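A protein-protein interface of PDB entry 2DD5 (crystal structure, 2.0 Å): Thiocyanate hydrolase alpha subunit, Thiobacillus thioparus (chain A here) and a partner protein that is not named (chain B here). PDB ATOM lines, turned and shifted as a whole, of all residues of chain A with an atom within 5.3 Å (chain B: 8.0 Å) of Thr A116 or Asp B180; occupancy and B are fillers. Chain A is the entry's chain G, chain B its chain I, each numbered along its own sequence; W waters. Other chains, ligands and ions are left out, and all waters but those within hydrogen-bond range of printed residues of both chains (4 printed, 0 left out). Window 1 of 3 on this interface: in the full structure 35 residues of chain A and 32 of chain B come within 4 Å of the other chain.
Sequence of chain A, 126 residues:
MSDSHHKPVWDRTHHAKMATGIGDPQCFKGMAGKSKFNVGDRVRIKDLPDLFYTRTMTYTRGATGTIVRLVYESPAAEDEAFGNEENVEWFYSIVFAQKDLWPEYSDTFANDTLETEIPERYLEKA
Thr B129 touches Met A57 (OG1 to CG, 3.6 Å).
Met A57 touches Asp B180.
OH of Tyr A59 touches CG1 of Val B156, 3.9 Å away.
Ser A93 touches Arg B114 (OG to NH1, 3.7 Å).
Leu A114 touches Val B156 (CD1 to CB, 3.7 Å).
Val B178 touches Leu A114 (O to CA, 3.2 Å).
O of Glu A115 touches CA of Ala B179, 3.3 Å away.
Water W3 lies within hydrogen-bond range of the side-chain carboxylate of Glu A115 (2.7 Å), the guanidinium group of Arg B114 (3.0 Å) and the guanidinium group of Arg B177 (3.5 Å).
Water W4 lies within hydrogen-bond range of O of Thr B185 (2.8 Å), N of Gln B183 (2.9 Å), OE1 of Glu A117 (3.4 Å) and N of Asn B182 (3.4 Å).
The backbone carbonyl oxygen (O) of Met A57 is in hydrogen-bond range of the side-chain hydroxyl (OG1) of Thr A60, 2.8 Å away.
The backbone NH (N) of Arg B114 lies within hydrogen-bond range of the backbone carbonyl oxygen (O) of Arg B186 (2.9 Å).
The backbone NH (N) of Ala B179 is in hydrogen-bond range of the backbone carbonyl oxygen (O) of Val B125 (3.0 Å).
O of Gln B183 lies within hydrogen-bond range of NH1 of Arg B186, at 2.8 Å.
Of the 24 printed residues of chain B, 10 touch a printed residue of chain A.
Hydrophobic or aromatic side chains of chain B that line the printed part of chain A: Val B156.
Among the printed residues, 18 pairs touch across the chains.
The side-chain sulfur (SD) of Met A57 is in hydrogen-bond range of the side-chain amide nitrogen (ND2) of Asn B182 (3.5 Å).
The side-chain hydroxyl (OH) of Tyr A59 is in hydrogen-bond range of the side-chain carboxylate (OD2) of Asp B180 (2.7 Å).
OE2 of Glu A115 lies within salt-bridge range of NH1 of Arg B114, at 2.9 Å.
OE1 of Glu A115 is in salt-bridge range of NH1 of Arg B177, 2.9 Å away.
The backbone NH (N) of Glu A115 lies within hydrogen-bond range of the backbone carbonyl oxygen (O) of Val B178, at 2.7 Å.
The backbone carbonyl oxygen of Glu A115 is in hydrogen-bond range of the backbone NH of Asp B180, 2.9 Å away.
The side-chain hydroxyl (OG1) of Thr A116 sits at hydrogen-bond distance from the backbone carbonyl oxygen (O) of Asp B180 (3.0 Å).
The side-chain hydroxyl (OG1) of Thr A116 is in hydrogen-bond range of the side-chain amide oxygen (OD1) of Asn B182 (2.7 Å).
The backbone carbonyl oxygen (O) of Glu A117 lies within hydrogen-bond range of the side-chain amide nitrogen (ND2) of Asn B182 (2.8 Å).
The backbone carbonyl oxygen (O) of Glu A117 lies within hydrogen-bond range of the side-chain amide nitrogen (NE2) of Gln B183, at 3.4 Å.
The side-chain hydroxyl (OG1) of Thr B185 is in hydrogen-bond range of the side-chain carboxylate (OE2) of Glu A117 (2.6 Å).
Printed residues of chain B within 4 Å of Met A57: Thr B129, Asp B180 and Asn B182.
Thr A116 touches two residues of chain B.
Of the printed residues of chain A, Thr B129 touches Met A57.
CSO B133 touches none of the printed residues of chain A.
Of the printed residues of chain A, Asp B180 touches Met A57 (3.5 Å), Tyr A59 (2.7 Å), Glu A115 (2.9 Å) and Thr A116 (3.0 Å).
The nearest printed residue of chain B that does not touch Leu A114 is Arg B177 (4.7 Å).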
ATOM      1  N   MET A  57       0.155 -31.494  30.492  1.00  0.00           N
ATOM      2  CA  MET A  57       0.946 -31.732  31.690  1.00  0.00           C
ATOM      3  C   MET A  57       0.202 -31.676  33.015  1.00  0.00           C
ATOM      4  O   MET A  57      -0.659 -30.821  33.238  1.00  0.00           O
ATOM      5  CB  MET A  57       2.130 -30.762  31.747  1.00  0.00           C
ATOM      6  CG  MET A  57       3.104 -30.861  30.572  1.00  0.00           C
ATOM      7  SD  MET A  57       2.410 -30.250  29.014  1.00  0.00           S
ATOM      8  CE  MET A  57       2.379 -28.484  29.318  1.00  0.00           C
ATOM      9  N   TYR A  59       1.302 -30.699  35.746  1.00  0.00           N
ATOM     10  CA  TYR A  59       1.562 -29.443  36.448  1.00  0.00           C
ATOM     11  C   TYR A  59       0.597 -28.302  36.128  1.00  0.00           C
ATOM     12  O   TYR A  59       0.555 -27.308  36.853  1.00  0.00           O
ATOM     13  CB  TYR A  59       3.034 -29.004  36.262  1.00  0.00           C
ATOM     14  CG  TYR A  59       3.424 -28.422  34.915  1.00  0.00           C
ATOM     15  CD1 TYR A  59       3.001 -27.145  34.532  1.00  0.00           C
ATOM     16  CD2 TYR A  59       4.255 -29.129  34.045  1.00  0.00           C
ATOM     17  CE1 TYR A  59       3.399 -26.583  33.311  1.00  0.00           C
ATOM     18  CE2 TYR A  59       4.660 -28.578  32.820  1.00  0.00           C
ATOM     19  CZ  TYR A  59       4.228 -27.307  32.463  1.00  0.00           C
ATOM     20  OH  TYR A  59       4.622 -26.764  31.260  1.00  0.00           O
ATOM     21  N   THR A  60      -0.202 -28.447  35.073  1.00  0.00           N
ATOM     22  CA  THR A  60      -1.167 -27.408  34.713  1.00  0.00           C
ATOM     23  C   THR A  60      -2.579 -27.664  35.257  1.00  0.00           C
ATOM     24  O   THR A  60      -3.381 -26.735  35.358  1.00  0.00           O
ATOM     25  CB  THR A  60      -1.325 -27.249  33.171  1.00  0.00           C
ATOM     26  OG1 THR A  60      -1.949 -28.422  32.629  1.00  0.00           O
ATOM     27  CG2 THR A  60       0.023 -27.024  32.501  1.00  0.00           C
ATOM     28  N   TYR A  92      -5.322 -23.839  22.026  1.00  0.00           N
ATOM     29  CA  TYR A  92      -5.088 -22.499  22.539  1.00  0.00           C
ATOM     30  C   TYR A  92      -3.745 -22.381  23.231  1.00  0.00           C
ATOM     31  O   TYR A  92      -3.291 -23.314  23.894  1.00  0.00           O
ATOM     32  CB  TYR A  92      -6.181 -22.133  23.548  1.00  0.00           C
ATOM     33  CG  TYR A  92      -7.595 -22.217  23.023  1.00  0.00           C
ATOM     34  CD1 TYR A  92      -8.291 -21.066  22.654  1.00  0.00           C
ATOM     35  CD2 TYR A  92      -8.255 -23.444  22.931  1.00  0.00           C
ATOM     36  CE1 TYR A  92      -9.614 -21.133  22.211  1.00  0.00           C
ATOM     37  CE2 TYR A  92      -9.576 -23.523  22.489  1.00  0.00           C
ATOM     38  CZ  TYR A  92     -10.249 -22.360  22.134  1.00  0.00           C
ATOM     39  OH  TYR A  92     -11.564 -22.422  21.730  1.00  0.00           O
ATOM     40  N   SER A  93      -3.104 -21.234  23.071  1.00  0.00           N
ATOM     41  CA  SER A  93      -1.841 -20.999  23.753  1.00  0.00           C
ATOM     42  C   SER A  93      -2.284 -20.274  25.022  1.00  0.00           C
ATOM     43  O   SER A  93      -2.986 -19.259  24.954  1.00  0.00           O
ATOM     44  CB  SER A  93      -0.923 -20.108  22.925  1.00  0.00           C
ATOM     45  OG  SER A  93       0.366 -20.074  23.507  1.00  0.00           O
ATOM     46  N   ILE A  94      -1.888 -20.801  26.173  1.00  0.00           N
ATOM     47  CA  ILE A  94      -2.294 -20.225  27.450  1.00  0.00           C
ATOM     48  C   ILE A  94      -1.106 -19.794  28.305  1.00  0.00           C
ATOM     49  O   ILE A  94      -0.101 -20.501  28.387  1.00  0.00           O
ATOM     50  CB  ILE A  94      -3.160 -21.254  28.221  1.00  0.00           C
ATOM     51  CG1 ILE A  94      -4.399 -21.588  27.387  1.00  0.00           C
ATOM     52  CG2 ILE A  94      -3.567 -20.707  29.591  1.00  0.00           C
ATOM     53  CD1 ILE A  94      -5.186 -22.775  27.885  1.00  0.00           C
ATOM     54  N   PHE A  96       0.323 -18.879  32.024  1.00  0.00           N
ATOM     55  CA  PHE A  96       0.117 -19.055  33.460  1.00  0.00           C
ATOM     56  C   PHE A  96       1.139 -18.229  34.231  1.00  0.00           C
ATOM     57  O   PHE A  96       2.273 -18.058  33.781  1.00  0.00           O
ATOM     58  CB  PHE A  96       0.334 -20.517  33.859  1.00  0.00           C
ATOM     59  CG  PHE A  96      -0.608 -21.481  33.206  1.00  0.00           C
ATOM     60  CD1 PHE A  96      -1.869 -21.707  33.738  1.00  0.00           C
ATOM     61  CD2 PHE A  96      -0.216 -22.193  32.077  1.00  0.00           C
ATOM     62  CE1 PHE A  96      -2.730 -22.633  33.159  1.00  0.00           C
ATOM     63  CE2 PHE A  96      -1.069 -23.121  31.488  1.00  0.00           C
ATOM     64  CZ  PHE A  96      -2.329 -23.342  32.031  1.00  0.00           C
ATOM     65  N   LEU A 114       4.586 -18.889  32.275  1.00  0.00           N
ATOM     66  CA  LEU A 114       4.824 -20.129  31.551  1.00  0.00           C
ATOM     67  C   LEU A 114       3.729 -20.214  30.505  1.00  0.00           C
ATOM     68  O   LEU A 114       2.549 -20.066  30.824  1.00  0.00           O
ATOM     69  CB  LEU A 114       4.751 -21.334  32.496  1.00  0.00           C
ATOM     70  CG  LEU A 114       4.998 -22.705  31.853  1.00  0.00           C
ATOM     71  CD1 LEU A 114       5.535 -23.660  32.900  1.00  0.00           C
ATOM     72  CD2 LEU A 114       3.710 -23.240  31.227  1.00  0.00           C
ATOM     73  N   GLU A 115       4.119 -20.440  29.254  1.00  0.00           N
ATOM     74  CA  GLU A 115       3.152 -20.530  28.166  1.00  0.00           C
ATOM     75  C   GLU A 115       3.214 -21.916  27.546  1.00  0.00           C
ATOM     76  O   GLU A 115       4.294 -22.464  27.330  1.00  0.00           O
ATOM     77  CB  GLU A 115       3.448 -19.471  27.094  1.00  0.00           C
ATOM     78  CG  GLU A 115       2.361 -19.365  26.027  1.00  0.00           C
ATOM     79  CD  GLU A 115       2.634 -18.280  24.991  1.00  0.00           C
ATOM     80  OE1 GLU A 115       3.480 -17.397  25.249  1.00  0.00           O
ATOM     81  OE2 GLU A 115       1.987 -18.304  23.917  1.00  0.00           O
ATOM     82  N   THR A 116       2.050 -22.486  27.267  1.00  0.00           N
ATOM     83  CA  THR A 116       1.992 -23.812  26.674  1.00  0.00           C
ATOM     84  C   THR A 116       0.649 -23.955  25.956  1.00  0.00           C
ATOM     85  O   THR A 116      -0.241 -23.121  26.128  1.00  0.00           O
ATOM     86  CB  THR A 116       2.190 -24.900  27.768  1.00  0.00           C
ATOM     87  OG1 THR A 116       2.384 -26.174  27.149  1.00  0.00           O
ATOM     88  CG2 THR A 116       0.992 -24.954  28.705  1.00  0.00           C
ATOM     89  N   GLU A 117       0.496 -24.996  25.146  1.00  0.00           N
ATOM     90  CA  GLU A 117      -0.744 -25.164  24.397  1.00  0.00           C
ATOM     91  C   GLU A 117      -1.632 -26.280  24.918  1.00  0.00           C
ATOM     92  O   GLU A 117      -1.155 -27.337  25.311  1.00  0.00           O
ATOM     93  CB  GLU A 117      -0.428 -25.384  22.915  1.00  0.00           C
ATOM     94  CG  GLU A 117       0.449 -24.284  22.336  1.00  0.00           C
ATOM     95  CD  GLU A 117       0.660 -24.403  20.838  1.00  0.00           C
ATOM     96  OE1 GLU A 117       0.635 -25.537  20.312  1.00  0.00           O
ATOM     97  OE2 GLU A 117       0.868 -23.353  20.192  1.00  0.00           O
ATOM     98  N   ILE A 118      -2.936 -26.031  24.902  1.00  0.00           N
ATOM     99  CA  ILE A 118      -3.901 -27.005  25.383  1.00  0.00           C
ATOM    100  C   ILE A 118      -5.135 -27.057  24.488  1.00  0.00           C
ATOM    101  O   ILE A 118      -5.668 -26.019  24.092  1.00  0.00           O
ATOM    102  CB  ILE A 118      -4.339 -26.656  26.833  1.00  0.00           C
ATOM    103  CG1 ILE A 118      -3.113 -26.659  27.755  1.00  0.00           C
ATOM    104  CG2 ILE A 118      -5.380 -27.655  27.325  1.00  0.00           C
ATOM    105  CD1 ILE A 118      -3.395 -26.224  29.172  1.00  0.00           C
ATOM    106  N   ARG B 114       6.545 -20.549  15.806  1.00  0.00           N
ATOM    107  CA  ARG B 114       6.186 -19.279  16.413  1.00  0.00           C
ATOM    108  C   ARG B 114       7.485 -18.655  16.894  1.00  0.00           C
ATOM    109  O   ARG B 114       8.368 -19.346  17.414  1.00  0.00           O
ATOM    110  CB  ARG B 114       5.226 -19.455  17.594  1.00  0.00           C
ATOM    111  CG  ARG B 114       3.766 -19.672  17.206  1.00  0.00           C
ATOM    112  CD  ARG B 114       2.863 -19.386  18.399  1.00  0.00           C
ATOM    113  NE  ARG B 114       3.029 -18.006  18.851  1.00  0.00           N
ATOM    114  CZ  ARG B 114       2.906 -17.599  20.113  1.00  0.00           C
ATOM    115  NH1 ARG B 114       2.609 -18.463  21.078  1.00  0.00           N
ATOM    116  NH2 ARG B 114       3.092 -16.318  20.411  1.00  0.00           N
ATOM    117  N   LEU B 116       9.199 -16.067  19.439  1.00  0.00           N
ATOM    118  CA  LEU B 116       8.972 -15.373  20.697  1.00  0.00           C
ATOM    119  C   LEU B 116       9.955 -14.216  20.807  1.00  0.00           C
ATOM    120  O   LEU B 116      11.159 -14.423  20.955  1.00  0.00           O
ATOM    121  CB  LEU B 116       9.168 -16.344  21.864  1.00  0.00           C
ATOM    122  CG  LEU B 116       8.370 -17.650  21.777  1.00  0.00           C
ATOM    123  CD1 LEU B 116       8.783 -18.584  22.913  1.00  0.00           C
ATOM    124  CD2 LEU B 116       6.873 -17.351  21.844  1.00  0.00           C
ATOM    125  N   VAL B 125      12.534 -18.660  27.129  1.00  0.00           N
ATOM    126  CA  VAL B 125      13.403 -19.834  27.126  1.00  0.00           C
ATOM    127  C   VAL B 125      12.460 -21.001  26.796  1.00  0.00           C
ATOM    128  O   VAL B 125      11.339 -21.061  27.299  1.00  0.00           O
ATOM    129  CB  VAL B 125      14.127 -20.038  28.474  1.00  0.00           C
ATOM    130  CG1 VAL B 125      13.128 -20.281  29.593  1.00  0.00           C
ATOM    131  CG2 VAL B 125      15.117 -21.194  28.343  1.00  0.00           C
ATOM    132  N   VAL B 126      12.917 -21.916  25.946  1.00  0.00           N
ATOM    133  CA  VAL B 126      12.079 -23.018  25.483  1.00  0.00           C
ATOM    134  C   VAL B 126      12.487 -24.414  25.944  1.00  0.00           C
ATOM    135  O   VAL B 126      13.658 -24.689  26.195  1.00  0.00           O
ATOM    136  CB  VAL B 126      12.025 -23.012  23.930  1.00  0.00           C
ATOM    137  CG1 VAL B 126      11.047 -24.075  23.417  1.00  0.00           C
ATOM    138  CG2 VAL B 126      11.619 -21.621  23.434  1.00  0.00           C
ATOM    139  N   VAL B 127      11.492 -25.290  26.039  1.00  0.00           N
ATOM    140  CA  VAL B 127      11.702 -26.672  26.444  1.00  0.00           C
ATOM    141  C   VAL B 127      10.505 -27.504  25.984  1.00  0.00           C
ATOM    142  O   VAL B 127       9.464 -26.955  25.627  1.00  0.00           O
ATOM    143  CB  VAL B 127      11.809 -26.792  27.996  1.00  0.00           C
ATOM    144  CG1 VAL B 127      10.516 -26.313  28.654  1.00  0.00           C
ATOM    145  CG2 VAL B 127      12.073 -28.246  28.401  1.00  0.00           C
ATOM    146  N   CYS B 128      10.682 -28.822  25.949  1.00  0.00           N
ATOM    147  CA  CYS B 128       9.594 -29.744  25.646  1.00  0.00           C
ATOM    148  C   CYS B 128       9.635 -30.689  26.848  1.00  0.00           C
ATOM    149  O   CYS B 128      10.406 -31.645  26.860  1.00  0.00           O
ATOM    150  CB  CYS B 128       9.841 -30.542  24.358  1.00  0.00           C
ATOM    151  SG  CYS B 128       8.533 -31.768  24.133  1.00  0.00           S
ATOM    152  N   THR B 129       8.842 -30.411  27.877  1.00  0.00           N
ATOM    153  CA  THR B 129       8.874 -31.260  29.061  1.00  0.00           C
ATOM    154  C   THR B 129       8.453 -32.692  28.764  1.00  0.00           C
ATOM    155  O   THR B 129       8.881 -33.615  29.453  1.00  0.00           O
ATOM    156  CB  THR B 129       7.987 -30.693  30.197  1.00  0.00           C
ATOM    157  OG1 THR B 129       6.616 -30.680  29.787  1.00  0.00           O
ATOM    158  CG2 THR B 129       8.426 -29.276  30.559  1.00  0.00           C
ATOM    159  N   LEU B 130       7.639 -32.882  27.728  1.00  0.00           N
ATOM    160  CA  LEU B 130       7.164 -34.221  27.377  1.00  0.00           C
ATOM    161  C   LEU B 130       8.152 -35.052  26.573  1.00  0.00           C
ATOM    162  O   LEU B 130       8.057 -36.283  26.561  1.00  0.00           O
ATOM    163  CB  LEU B 130       5.826 -34.131  26.625  1.00  0.00           C
ATOM    164  CG  LEU B 130       4.680 -33.489  27.425  1.00  0.00           C
ATOM    165  CD1 LEU B 130       3.394 -33.483  26.608  1.00  0.00           C
ATOM    166  CD2 LEU B 130       4.475 -34.264  28.725  1.00  0.00           C
ATOM    167  N   CSD B 131       9.088 -34.383  25.895  1.00  0.00           N
ATOM    168  CA  CSD B 131      10.091 -35.068  25.085  1.00  0.00           C
ATOM    169  CB  CSD B 131       9.483 -35.933  23.970  1.00  0.00           C
ATOM    170  SG  CSD B 131       8.147 -35.097  23.031  1.00  0.00           S
ATOM    171  C   CSD B 131      11.362 -34.335  24.662  1.00  0.00           C
ATOM    172  O   CSD B 131      12.341 -34.270  25.408  1.00  0.00           O
ATOM    173  N   CSO B 133      10.746 -31.985  21.617  1.00  0.00           N
ATOM    174  CA  CSO B 133      10.198 -31.136  20.577  1.00  0.00           C
ATOM    175  CB  CSO B 133       8.696 -30.916  20.739  1.00  0.00           C
ATOM    176  SG  CSO B 133       7.794 -32.505  20.964  1.00  0.00           S
ATOM    177  C   CSO B 133      11.034 -29.873  20.335  1.00  0.00           C
ATOM    178  O   CSO B 133      11.221 -29.057  21.241  1.00  0.00           O
ATOM    179  N   TYR B 146      19.121 -30.752  26.151  1.00  0.00           N
ATOM    180  CA  TYR B 146      17.747 -30.298  25.940  1.00  0.00           C
ATOM    181  C   TYR B 146      16.784 -31.485  26.043  1.00  0.00           C
ATOM    182  O   TYR B 146      15.626 -31.337  26.452  1.00  0.00           O
ATOM    183  CB  TYR B 146      17.635 -29.652  24.555  1.00  0.00           C
ATOM    184  CG  TYR B 146      16.271 -29.090  24.204  1.00  0.00           C
ATOM    185  CD1 TYR B 146      15.934 -27.772  24.516  1.00  0.00           C
ATOM    186  CD2 TYR B 146      15.333 -29.867  23.524  1.00  0.00           C
ATOM    187  CE1 TYR B 146      14.688 -27.238  24.148  1.00  0.00           C
ATOM    188  CE2 TYR B 146      14.089 -29.348  23.157  1.00  0.00           C
ATOM    189  CZ  TYR B 146      13.775 -28.030  23.471  1.00  0.00           C
ATOM    190  OH  TYR B 146      12.547 -27.519  23.111  1.00  0.00           O
ATOM    191  N   ARG B 152      14.122 -31.140  31.345  1.00  0.00           N
ATOM    192  CA  ARG B 152      12.675 -31.212  31.162  1.00  0.00           C
ATOM    193  C   ARG B 152      11.906 -31.144  32.483  1.00  0.00           C
ATOM    194  O   ARG B 152      10.743 -30.747  32.523  1.00  0.00           O
ATOM    195  CB  ARG B 152      12.326 -32.489  30.395  1.00  0.00           C
ATOM    196  CG  ARG B 152      12.863 -32.494  28.948  1.00  0.00           C
ATOM    197  CD  ARG B 152      12.788 -33.898  28.366  1.00  0.00           C
ATOM    198  NE  ARG B 152      11.475 -34.471  28.633  1.00  0.00           N
ATOM    199  CZ  ARG B 152      11.256 -35.758  28.879  1.00  0.00           C
ATOM    200  NH1 ARG B 152      12.266 -36.620  28.883  1.00  0.00           N
ATOM    201  NH2 ARG B 152      10.030 -36.171  29.164  1.00  0.00           N
ATOM    202  N   LEU B 155      13.440 -26.758  34.215  1.00  0.00           N
ATOM    203  CA  LEU B 155      13.210 -25.445  33.613  1.00  0.00           C
ATOM    204  C   LEU B 155      11.855 -24.801  33.870  1.00  0.00           C
ATOM    205  O   LEU B 155      11.785 -23.615  34.210  1.00  0.00           O
ATOM    206  CB  LEU B 155      13.460 -25.488  32.101  1.00  0.00           C
ATOM    207  CG  LEU B 155      13.423 -24.092  31.460  1.00  0.00           C
ATOM    208  CD1 LEU B 155      14.661 -23.320  31.886  1.00  0.00           C
ATOM    209  CD2 LEU B 155      13.370 -24.204  29.941  1.00  0.00           C
ATOM    210  N   VAL B 156      10.774 -25.557  33.714  1.00  0.00           N
ATOM    211  CA  VAL B 156       9.454 -24.977  33.916  1.00  0.00           C
ATOM    212  C   VAL B 156       9.169 -24.503  35.338  1.00  0.00           C
ATOM    213  O   VAL B 156       8.328 -23.631  35.538  1.00  0.00           O
ATOM    214  CB  VAL B 156       8.330 -25.956  33.487  1.00  0.00           C
ATOM    215  CG1 VAL B 156       8.446 -26.255  32.003  1.00  0.00           C
ATOM    216  CG2 VAL B 156       8.406 -27.256  34.302  1.00  0.00           C
ATOM    217  N   ARG B 177       9.617 -15.869  30.657  1.00  0.00           N
ATOM    218  CA  ARG B 177       8.535 -16.725  30.208  1.00  0.00           C
ATOM    219  C   ARG B 177       9.090 -18.027  29.651  1.00  0.00           C
ATOM    220  O   ARG B 177       9.880 -18.025  28.705  1.00  0.00           O
ATOM    221  CB  ARG B 177       7.686 -16.038  29.131  1.00  0.00           C
ATOM    222  CG  ARG B 177       6.621 -16.964  28.548  1.00  0.00           C
ATOM    223  CD  ARG B 177       5.627 -16.250  27.650  1.00  0.00           C
ATOM    224  NE  ARG B 177       4.890 -15.209  28.361  1.00  0.00           N
ATOM    225  CZ  ARG B 177       3.868 -14.532  27.846  1.00  0.00           C
ATOM    226  NH1 ARG B 177       3.449 -14.792  26.612  1.00  0.00           N
ATOM    227  NH2 ARG B 177       3.281 -13.573  28.552  1.00  0.00           N
ATOM    228  N   VAL B 178       8.685 -19.134  30.260  1.00  0.00           N
ATOM    229  CA  VAL B 178       9.110 -20.444  29.800  1.00  0.00           C
ATOM    230  C   VAL B 178       8.023 -20.927  28.852  1.00  0.00           C
ATOM    231  O   VAL B 178       6.834 -20.834  29.172  1.00  0.00           O
ATOM    232  CB  VAL B 178       9.220 -21.456  30.966  1.00  0.00           C
ATOM    233  CG1 VAL B 178       9.628 -22.823  30.427  1.00  0.00           C
ATOM    234  CG2 VAL B 178      10.237 -20.971  31.986  1.00  0.00           C
ATOM    235  N   ALA B 179       8.423 -21.408  27.677  1.00  0.00           N
ATOM    236  CA  ALA B 179       7.465 -21.925  26.709  1.00  0.00           C
ATOM    237  C   ALA B 179       7.651 -23.438  26.633  1.00  0.00           C
ATOM    238  O   ALA B 179       8.745 -23.918  26.341  1.00  0.00           O
ATOM    239  CB  ALA B 179       7.694 -21.292  25.332  1.00  0.00           C
ATOM    240  N   ASP B 180       6.587 -24.186  26.913  1.00  0.00           N
ATOM    241  CA  ASP B 180       6.656 -25.644  26.865  1.00  0.00           C
ATOM    242  C   ASP B 180       6.027 -26.101  25.549  1.00  0.00           C
ATOM    243  O   ASP B 180       4.818 -25.965  25.359  1.00  0.00           O
ATOM    244  CB  ASP B 180       5.889 -26.251  28.047  1.00  0.00           C
ATOM    245  CG  ASP B 180       6.190 -27.728  28.248  1.00  0.00           C
ATOM    246  OD1 ASP B 180       6.773 -28.360  27.332  1.00  0.00           O
ATOM    247  OD2 ASP B 180       5.837 -28.262  29.324  1.00  0.00           O
ATOM    248  N   SER B 181       6.848 -26.635  24.645  1.00  0.00           N
ATOM    249  CA  SER B 181       6.368 -27.101  23.337  1.00  0.00           C
ATOM    250  C   SER B 181       5.723 -28.473  23.467  1.00  0.00           C
ATOM    251  O   SER B 181       6.333 -29.477  23.108  1.00  0.00           O
ATOM    252  CB  SER B 181       7.537 -27.205  22.355  1.00  0.00           C
ATOM    253  OG  SER B 181       8.454 -26.145  22.546  1.00  0.00           O
ATOM    254  N   ASN B 182       4.484 -28.514  23.945  1.00  0.00           N
ATOM    255  CA  ASN B 182       3.789 -29.782  24.161  1.00  0.00           C
ATOM    256  C   ASN B 182       2.798 -30.230  23.089  1.00  0.00           C
ATOM    257  O   ASN B 182       2.202 -31.298  23.217  1.00  0.00           O
ATOM    258  CB  ASN B 182       3.061 -29.726  25.499  1.00  0.00           C
ATOM    259  CG  ASN B 182       1.935 -28.723  25.492  1.00  0.00           C
ATOM    260  OD1 ASN B 182       2.052 -27.656  24.895  1.00  0.00           O
ATOM    261  ND2 ASN B 182       0.838 -29.053  26.159  1.00  0.00           N
ATOM    262  N   GLN B 183       2.592 -29.425  22.050  1.00  0.00           N
ATOM    263  CA  GLN B 183       1.667 -29.822  20.994  1.00  0.00           C
ATOM    264  C   GLN B 183       2.357 -29.700  19.631  1.00  0.00           C
ATOM    265  O   GLN B 183       3.498 -30.134  19.476  1.00  0.00           O
ATOM    266  CB  GLN B 183       0.379 -28.980  21.039  1.00  0.00           C
ATOM    267  CG  GLN B 183      -0.390 -28.995  22.387  1.00  0.00           C
ATOM    268  CD  GLN B 183      -0.935 -30.368  22.807  1.00  0.00           C
ATOM    269  OE1 GLN B 183      -1.058 -31.292  21.999  1.00  0.00           O
ATOM    270  NE2 GLN B 183      -1.285 -30.490  24.088  1.00  0.00           N
ATOM    271  N   THR B 185       3.158 -26.792  17.981  1.00  0.00           N
ATOM    272  CA  THR B 185       3.914 -25.563  17.771  1.00  0.00           C
ATOM    273  C   THR B 185       5.364 -25.731  18.212  1.00  0.00           C
ATOM    274  O   THR B 185       5.640 -26.396  19.209  1.00  0.00           O
ATOM    275  CB  THR B 185       3.301 -24.387  18.561  1.00  0.00           C
ATOM    276  OG1 THR B 185       2.056 -24.008  17.966  1.00  0.00           O
ATOM    277  CG2 THR B 185       4.241 -23.192  18.566  1.00  0.00           C
ATOM    278  N   ARG B 186       6.287 -25.149  17.451  1.00  0.00           N
ATOM    279  CA  ARG B 186       7.705 -25.181  17.790  1.00  0.00           C
ATOM    280  C   ARG B 186       8.121 -23.718  17.899  1.00  0.00           C
ATOM    281  O   ARG B 186       7.566 -22.862  17.203  1.00  0.00           O
ATOM    282  CB  ARG B 186       8.512 -25.888  16.698  1.00  0.00           C
ATOM    283  CG  ARG B 186       8.123 -27.348  16.500  1.00  0.00           C
ATOM    284  CD  ARG B 186       8.517 -28.208  17.705  1.00  0.00           C
ATOM    285  NE  ARG B 186       8.079 -29.594  17.554  1.00  0.00           N
ATOM    286  CZ  ARG B 186       6.879 -30.050  17.905  1.00  0.00           C
ATOM    287  NH1 ARG B 186       5.980 -29.233  18.443  1.00  0.00           N
ATOM    288  NH2 ARG B 186       6.575 -31.331  17.714  1.00  0.00           N
ATOM    289  N   TYR B 187       9.091 -23.424  18.763  1.00  0.00           N
ATOM    290  CA  TYR B 187       9.525 -22.044  18.966  1.00  0.00           C
ATOM    291  C   TYR B 187      11.010 -21.779  18.801  1.00  0.00           C
ATOM    292  O   TYR B 187      11.847 -22.666  18.973  1.00  0.00           O
ATOM    293  CB  TYR B 187       9.202 -21.573  20.393  1.00  0.00           C
ATOM    294  CG  TYR B 187       7.813 -21.841  20.911  1.00  0.00           C
ATOM    295  CD1 TYR B 187       6.780 -20.920  20.714  1.00  0.00           C
ATOM    296  CD2 TYR B 187       7.541 -22.989  21.656  1.00  0.00           C
ATOM    297  CE1 TYR B 187       5.516 -21.132  21.256  1.00  0.00           C
ATOM    298  CE2 TYR B 187       6.277 -23.214  22.197  1.00  0.00           C
ATOM    299  CZ  TYR B 187       5.273 -22.282  21.998  1.00  0.00           C
ATOM    300  OH  TYR B 187       4.034 -22.490  22.551  1.00  0.00           O
HETATM  301  O   HOH W   1       1.923 -21.231  21.452  1.00  0.00           O
HETATM  302  O   HOH W   2       3.352 -25.102  23.136  1.00  0.00           O
HETATM  303  O   HOH W   3       3.577 -15.592  23.251  1.00  0.00           O
HETATM  304  O   HOH W   4       3.603 -26.924  21.034  1.00  0.00           O
